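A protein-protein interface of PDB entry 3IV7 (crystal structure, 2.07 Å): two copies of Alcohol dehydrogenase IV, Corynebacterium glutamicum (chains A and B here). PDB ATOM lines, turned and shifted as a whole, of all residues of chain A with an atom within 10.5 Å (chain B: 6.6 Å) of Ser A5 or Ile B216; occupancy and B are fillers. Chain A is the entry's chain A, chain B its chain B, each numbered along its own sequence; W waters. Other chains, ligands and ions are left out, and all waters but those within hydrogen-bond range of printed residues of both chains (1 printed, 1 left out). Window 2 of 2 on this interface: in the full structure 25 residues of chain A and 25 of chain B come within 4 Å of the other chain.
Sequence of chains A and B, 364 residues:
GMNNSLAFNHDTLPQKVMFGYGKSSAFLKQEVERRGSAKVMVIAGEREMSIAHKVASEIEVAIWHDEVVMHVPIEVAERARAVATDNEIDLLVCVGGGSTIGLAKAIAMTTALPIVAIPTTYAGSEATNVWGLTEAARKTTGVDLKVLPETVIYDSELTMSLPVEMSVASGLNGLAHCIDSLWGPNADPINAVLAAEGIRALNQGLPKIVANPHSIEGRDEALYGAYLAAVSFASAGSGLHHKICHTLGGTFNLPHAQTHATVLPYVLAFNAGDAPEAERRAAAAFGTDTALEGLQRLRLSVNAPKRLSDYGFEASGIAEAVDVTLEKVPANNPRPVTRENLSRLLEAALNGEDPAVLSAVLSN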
ATOM      1  N   ASN A   4      -4.089   7.105   2.633  1.00  0.00           N
ATOM      2  CA  ASN A   4      -5.019   8.153   3.109  1.00  0.00           C
ATOM      3  C   ASN A   4      -5.128   8.179   4.645  1.00  0.00           C
ATOM      4  O   ASN A   4      -6.184   8.507   5.195  1.00  0.00           O
ATOM      5  CB  ASN A   4      -6.403   7.939   2.483  1.00  0.00           C
ATOM      6  N   SER A   5      -4.025   7.880   5.332  1.00  0.00           N
ATOM      7  CA  SER A   5      -4.010   7.838   6.808  1.00  0.00           C
ATOM      8  C   SER A   5      -4.021   9.236   7.429  1.00  0.00           C
ATOM      9  O   SER A   5      -3.904  10.232   6.733  1.00  0.00           O
ATOM     10  CB  SER A   5      -2.791   7.046   7.304  1.00  0.00           C
ATOM     11  OG  SER A   5      -1.572   7.655   6.905  1.00  0.00           O
ATOM     12  N   LEU A   6      -4.189   9.302   8.744  1.00  0.00           N
ATOM     13  CA  LEU A   6      -4.257  10.568   9.438  1.00  0.00           C
ATOM     14  C   LEU A   6      -2.994  11.428   9.243  1.00  0.00           C
ATOM     15  O   LEU A   6      -1.864  10.990   9.506  1.00  0.00           O
ATOM     16  CB  LEU A   6      -4.494  10.341  10.930  1.00  0.00           C
ATOM     17  CG  LEU A   6      -4.675  11.601  11.786  1.00  0.00           C
ATOM     18  CD1 LEU A   6      -5.687  12.546  11.146  1.00  0.00           C
ATOM     19  CD2 LEU A   6      -5.101  11.210  13.212  1.00  0.00           C
ATOM     20  N   ALA A   7      -3.198  12.653   8.800  1.00  0.00           N
ATOM     21  CA  ALA A   7      -2.111  13.562   8.573  1.00  0.00           C
ATOM     22  C   ALA A   7      -2.564  14.959   8.850  1.00  0.00           C
ATOM     23  O   ALA A   7      -3.621  15.366   8.384  1.00  0.00           O
ATOM     24  CB  ALA A   7      -1.626  13.440   7.146  1.00  0.00           C
ATOM     25  N   PHE A   8      -1.773  15.699   9.627  1.00  0.00           N
ATOM     26  CA  PHE A   8      -2.057  17.084   9.914  1.00  0.00           C
ATOM     27  C   PHE A   8      -0.852  17.851  10.456  1.00  0.00           C
ATOM     28  O   PHE A   8       0.160  17.270  10.861  1.00  0.00           O
ATOM     29  CB  PHE A   8      -3.253  17.227  10.885  1.00  0.00           C
ATOM     30  CG  PHE A   8      -3.018  16.639  12.258  1.00  0.00           C
ATOM     31  CD1 PHE A   8      -3.393  15.323  12.545  1.00  0.00           C
ATOM     32  CD2 PHE A   8      -2.486  17.426  13.296  1.00  0.00           C
ATOM     33  CE1 PHE A   8      -3.186  14.788  13.833  1.00  0.00           C
ATOM     34  CE2 PHE A   8      -2.249  16.874  14.576  1.00  0.00           C
ATOM     35  CZ  PHE A   8      -2.622  15.590  14.850  1.00  0.00           C
ATOM     36  N   ASN A   9      -0.949  19.168  10.361  1.00  0.00           N
ATOM     37  CA  ASN A   9       0.035  20.097  10.884  1.00  0.00           C
ATOM     38  C   ASN A   9      -0.762  21.105  11.720  1.00  0.00           C
ATOM     39  O   ASN A   9      -1.546  21.911  11.180  1.00  0.00           O
ATOM     40  CB  ASN A   9       0.765  20.778   9.718  1.00  0.00           C
ATOM     41  CG  ASN A   9       1.970  21.627  10.173  1.00  0.00           C
ATOM     42  OD1 ASN A   9       1.977  22.180  11.266  1.00  0.00           O
ATOM     43  ND2 ASN A   9       2.973  21.752   9.297  1.00  0.00           N
ATOM     44  N   ALA A 187      -8.879  21.975   8.769  1.00  0.00           N
ATOM     45  CA  ALA A 187      -9.548  21.160   9.735  1.00  0.00           C
ATOM     46  C   ALA A 187      -8.588  20.047  10.157  1.00  0.00           C
ATOM     47  O   ALA A 187      -7.893  19.457   9.319  1.00  0.00           O
ATOM     48  CB  ALA A 187     -10.858  20.537   9.108  1.00  0.00           C
ATOM     49  N   PRO A 189      -7.974  16.938  13.791  1.00  0.00           N
ATOM     50  CA  PRO A 189      -8.727  16.330  14.887  1.00  0.00           C
ATOM     51  C   PRO A 189      -8.816  17.149  16.142  1.00  0.00           C
ATOM     52  O   PRO A 189      -9.772  16.967  16.919  1.00  0.00           O
ATOM     53  CB  PRO A 189      -7.965  15.004  15.165  1.00  0.00           C
ATOM     54  CG  PRO A 189      -7.291  14.679  13.894  1.00  0.00           C
ATOM     55  CD  PRO A 189      -6.957  16.008  13.235  1.00  0.00           C
ATOM     56  N   GLU A 277     -18.523  12.910   8.389  1.00  0.00           N
ATOM     57  CA  GLU A 277     -17.829  12.876   9.677  1.00  0.00           C
ATOM     58  C   GLU A 277     -18.104  14.166  10.452  1.00  0.00           C
ATOM     59  O   GLU A 277     -18.397  14.123  11.639  1.00  0.00           O
ATOM     60  CB  GLU A 277     -16.319  12.652   9.492  1.00  0.00           C
ATOM     61  CG  GLU A 277     -15.984  11.292   8.841  1.00  0.00           C
ATOM     62  CD  GLU A 277     -14.504  10.896   8.949  1.00  0.00           C
ATOM     63  OE1 GLU A 277     -13.808  11.349   9.891  1.00  0.00           O
ATOM     64  OE2 GLU A 277     -14.053  10.080   8.110  1.00  0.00           O
ATOM     65  N   GLY B  20       1.995  12.307  10.883  1.00  0.00           N
ATOM     66  CA  GLY B  20       1.776  11.504   9.691  1.00  0.00           C
ATOM     67  C   GLY B  20       2.667  10.293   9.513  1.00  0.00           C
ATOM     68  O   GLY B  20       3.893  10.388   9.625  1.00  0.00           O
ATOM     69  N   TYR B  21       2.050   9.156   9.175  1.00  0.00           N
ATOM     70  CA  TYR B  21       2.802   7.899   8.968  1.00  0.00           C
ATOM     71  C   TYR B  21       3.768   8.064   7.823  1.00  0.00           C
ATOM     72  O   TYR B  21       3.381   8.504   6.753  1.00  0.00           O
ATOM     73  CB  TYR B  21       1.838   6.733   8.665  1.00  0.00           C
ATOM     74  CG  TYR B  21       2.525   5.422   8.260  1.00  0.00           C
ATOM     75  CD1 TYR B  21       2.735   5.105   6.924  1.00  0.00           C
ATOM     76  CD2 TYR B  21       2.935   4.508   9.218  1.00  0.00           C
ATOM     77  CE1 TYR B  21       3.346   3.879   6.542  1.00  0.00           C
ATOM     78  CE2 TYR B  21       3.544   3.296   8.856  1.00  0.00           C
ATOM     79  CZ  TYR B  21       3.755   2.998   7.520  1.00  0.00           C
ATOM     80  OH  TYR B  21       4.363   1.812   7.188  1.00  0.00           O
ATOM     81  N   SER B 156       3.947   7.514  13.254  1.00  0.00           N
ATOM     82  CA  SER B 156       3.604   6.232  13.854  1.00  0.00           C
ATOM     83  C   SER B 156       4.511   5.046  13.408  1.00  0.00           C
ATOM     84  O   SER B 156       4.609   4.043  14.122  1.00  0.00           O
ATOM     85  CB  SER B 156       2.142   5.913  13.603  1.00  0.00           C
ATOM     86  OG  SER B 156       1.864   5.849  12.205  1.00  0.00           O
ATOM     87  N   MET B 160       6.281   1.367  15.667  1.00  0.00           N
ATOM     88  CA  MET B 160       5.857  -0.003  15.324  1.00  0.00           C
ATOM     89  C   MET B 160       6.789  -1.111  15.794  1.00  0.00           C
ATOM     90  O   MET B 160       6.349  -2.238  15.993  1.00  0.00           O
ATOM     91  CB  MET B 160       5.560  -0.118  13.833  1.00  0.00           C
ATOM     92  CG  MET B 160       4.251   0.564  13.464  1.00  0.00           C
ATOM     93  SD  MET B 160       3.929   0.596  11.609  1.00  0.00           S
ATOM     94  CE  MET B 160       2.283   1.646  11.583  1.00  0.00           C
ATOM     95  N   ASN B 212      -2.541  -5.978  15.894  1.00  0.00           N
ATOM     96  CA  ASN B 212      -1.629  -5.731  14.781  1.00  0.00           C
ATOM     97  C   ASN B 212      -0.666  -4.590  15.109  1.00  0.00           C
ATOM     98  O   ASN B 212      -0.991  -3.426  14.889  1.00  0.00           O
ATOM     99  CB  ASN B 212      -2.424  -5.414  13.510  1.00  0.00           C
ATOM    100  CG  ASN B 212      -1.531  -5.043  12.339  1.00  0.00           C
ATOM    101  OD1 ASN B 212      -0.292  -5.139  12.426  1.00  0.00           O
ATOM    102  ND2 ASN B 212      -2.146  -4.587  11.242  1.00  0.00           N
ATOM    103  N   PRO B 213       0.542  -4.932  15.612  1.00  0.00           N
ATOM    104  CA  PRO B 213       1.561  -3.960  16.005  1.00  0.00           C
ATOM    105  C   PRO B 213       2.001  -3.012  14.885  1.00  0.00           C
ATOM    106  O   PRO B 213       2.628  -1.994  15.166  1.00  0.00           O
ATOM    107  CB  PRO B 213       2.738  -4.844  16.434  1.00  0.00           C
ATOM    108  CG  PRO B 213       2.137  -6.103  16.817  1.00  0.00           C
ATOM    109  CD  PRO B 213       0.936  -6.301  15.978  1.00  0.00           C
ATOM    110  N   HIS B 214       1.723  -3.365  13.631  1.00  0.00           N
ATOM    111  CA  HIS B 214       2.023  -2.474  12.523  1.00  0.00           C
ATOM    112  C   HIS B 214       0.766  -1.824  11.971  1.00  0.00           C
ATOM    113  O   HIS B 214       0.756  -1.340  10.849  1.00  0.00           O
ATOM    114  CB  HIS B 214       2.764  -3.210  11.442  1.00  0.00           C
ATOM    115  CG  HIS B 214       4.131  -3.663  11.852  1.00  0.00           C
ATOM    116  ND1 HIS B 214       4.351  -4.842  12.516  1.00  0.00           N
ATOM    117  CD2 HIS B 214       5.347  -3.096  11.678  1.00  0.00           C
ATOM    118  CE1 HIS B 214       5.643  -4.981  12.747  1.00  0.00           C
ATOM    119  NE2 HIS B 214       6.268  -3.928  12.255  1.00  0.00           N
ATOM    120  N   SER B 215      -0.273  -1.753  12.798  1.00  0.00           N
ATOM    121  CA  SER B 215      -1.515  -1.113  12.405  1.00  0.00           C
ATOM    122  C   SER B 215      -1.327   0.389  12.301  1.00  0.00           C
ATOM    123  O   SER B 215      -1.029   1.045  13.284  1.00  0.00           O
ATOM    124  CB  SER B 215      -2.618  -1.409  13.405  1.00  0.00           C
ATOM    125  OG  SER B 215      -3.770  -0.643  13.092  1.00  0.00           O
ATOM    126  N   ILE B 216      -1.493   0.929  11.098  1.00  0.00           N
ATOM    127  CA  ILE B 216      -1.346   2.349  10.893  1.00  0.00           C
ATOM    128  C   ILE B 216      -2.439   3.077  11.668  1.00  0.00           C
ATOM    129  O   ILE B 216      -2.157   3.975  12.462  1.00  0.00           O
ATOM    130  CB  ILE B 216      -1.406   2.706   9.409  1.00  0.00           C
ATOM    131  CG1 ILE B 216      -0.170   2.108   8.680  1.00  0.00           C
ATOM    132  CG2 ILE B 216      -1.471   4.214   9.253  1.00  0.00           C
ATOM    133  CD1 ILE B 216      -0.340   1.910   7.144  1.00  0.00           C
ATOM    134  N   GLU B 217      -3.682   2.652  11.468  1.00  0.00           N
ATOM    135  CA  GLU B 217      -4.808   3.244  12.162  1.00  0.00           C
ATOM    136  C   GLU B 217      -4.632   3.206  13.689  1.00  0.00           C
ATOM    137  O   GLU B 217      -4.796   4.213  14.360  1.00  0.00           O
ATOM    138  CB  GLU B 217      -6.094   2.513  11.773  1.00  0.00           C
ATOM    139  CG  GLU B 217      -7.337   3.046  12.449  1.00  0.00           C
ATOM    140  CD  GLU B 217      -8.575   2.254  12.054  1.00  0.00           C
ATOM    141  OE1 GLU B 217      -8.714   1.923  10.859  1.00  0.00           O
ATOM    142  OE2 GLU B 217      -9.393   1.951  12.932  1.00  0.00           O
ATOM    143  N   GLY B 218      -4.323   2.035  14.222  1.00  0.00           N
ATOM    144  CA  GLY B 218      -4.173   1.872  15.662  1.00  0.00           C
ATOM    145  C   GLY B 218      -2.977   2.579  16.256  1.00  0.00           C
ATOM    146  O   GLY B 218      -3.076   3.172  17.337  1.00  0.00           O
ATOM    147  N   ARG B 219      -1.832   2.501  15.592  1.00  0.00           N
ATOM    148  CA  ARG B 219      -0.656   3.202  16.088  1.00  0.00           C
ATOM    149  C   ARG B 219      -0.857   4.730  15.993  1.00  0.00           C
ATOM    150  O   ARG B 219      -0.319   5.496  16.834  1.00  0.00           O
ATOM    151  CB  ARG B 219       0.601   2.804  15.332  1.00  0.00           C
ATOM    152  CG  ARG B 219       1.111   1.386  15.598  1.00  0.00           C
ATOM    153  CD  ARG B 219       1.727   1.227  17.025  1.00  0.00           C
ATOM    154  NE  ARG B 219       2.488  -0.002  17.130  1.00  0.00           N
ATOM    155  CZ  ARG B 219       3.175  -0.393  18.199  1.00  0.00           C
ATOM    156  NH1 ARG B 219       3.233   0.364  19.299  1.00  0.00           N
ATOM    157  NH2 ARG B 219       3.847  -1.532  18.153  1.00  0.00           N
ATOM    158  N   ASP B 220      -1.586   5.186  14.967  1.00  0.00           N
ATOM    159  CA  ASP B 220      -1.875   6.638  14.853  1.00  0.00           C
ATOM    160  C   ASP B 220      -2.772   7.093  16.035  1.00  0.00           C
ATOM    161  O   ASP B 220      -2.525   8.131  16.657  1.00  0.00           O
ATOM    162  CB  ASP B 220      -2.563   6.985  13.519  1.00  0.00           C
ATOM    163  CG  ASP B 220      -1.583   7.120  12.352  1.00  0.00           C
ATOM    164  OD1 ASP B 220      -0.362   7.142  12.577  1.00  0.00           O
ATOM    165  OD2 ASP B 220      -2.046   7.232  11.202  1.00  0.00           O
ATOM    166  N   GLU B 221      -3.825   6.336  16.309  1.00  0.00           N
ATOM    167  CA  GLU B 221      -4.740   6.677  17.392  1.00  0.00           C
ATOM    168  C   GLU B 221      -4.025   6.740  18.734  1.00  0.00           C
ATOM    169  O   GLU B 221      -4.240   7.667  19.528  1.00  0.00           O
ATOM    170  CB  GLU B 221      -5.908   5.671  17.436  1.00  0.00           C
ATOM    171  CG  GLU B 221      -6.864   5.876  16.291  1.00  0.00           C
ATOM    172  CD  GLU B 221      -7.958   4.838  16.196  1.00  0.00           C
ATOM    173  OE1 GLU B 221      -7.716   3.655  16.523  1.00  0.00           O
ATOM    174  OE2 GLU B 221      -9.051   5.199  15.703  1.00  0.00           O
HETATM  175  O   HOH W   1      -4.782   6.803  10.646  1.00  0.00           O
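No position is printed for both chains.
Of the 9 printed residues of chain A, 2 touch a printed residue of chain B.
Hydrophobic or aromatic side chains of chain B within 4 Å of the printed part of chain A: Tyr B21 and Ile B216.
Among the printed residues, 5 pairs touch across the chains.
Among the printed residues, no Asp or Glu carboxylate lies within 4 Å of a Lys or Arg side-chain nitrogen of the other chain.
Among the printed residues, merely in contact across the chains: Ser A5 with Tyr B21, Ser A5 with Ile B216, Ser A5 with Asp B220, Leu A6 with Gly B20 and Leu A6 with Asp B220.
Water W1 lies within hydrogen-bond range of the side-chain carboxylate of Asp B220 (2.8 Å) and the backbone NH of Leu A6 (3.2 Å).
Ser A5 touches three residues of chain B.
Of the printed residues of chain B, Leu A6 touches Gly B20 and Asp B220.
Of the printed residues of chain A, Gly B20 touches Leu A6 (3.7 Å).
Of chain A, only Ser A5 (3.9 Å) comes within 4 Å of Tyr B21.
Ser B215 touches none of the printed residues of chain A.
Of chain A, only Ser A5 (3.7 Å) comes within 4 Å of Ile B216.
No residue of chain A comes within 4 Å of Gly B218.
The nearest residue of chain B that does not touch Ser A5 is Gly B20 (5.6 Å).
The nearest printed residue of chain B that does not touch Leu A6 is Tyr B21 (4.3 Å).
The side-chain carboxylate (OD1) of Asp B220 lies within hydrogen-bond range of the side-chain hydroxyl (OG) of Ser B156 (2.6 Å).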
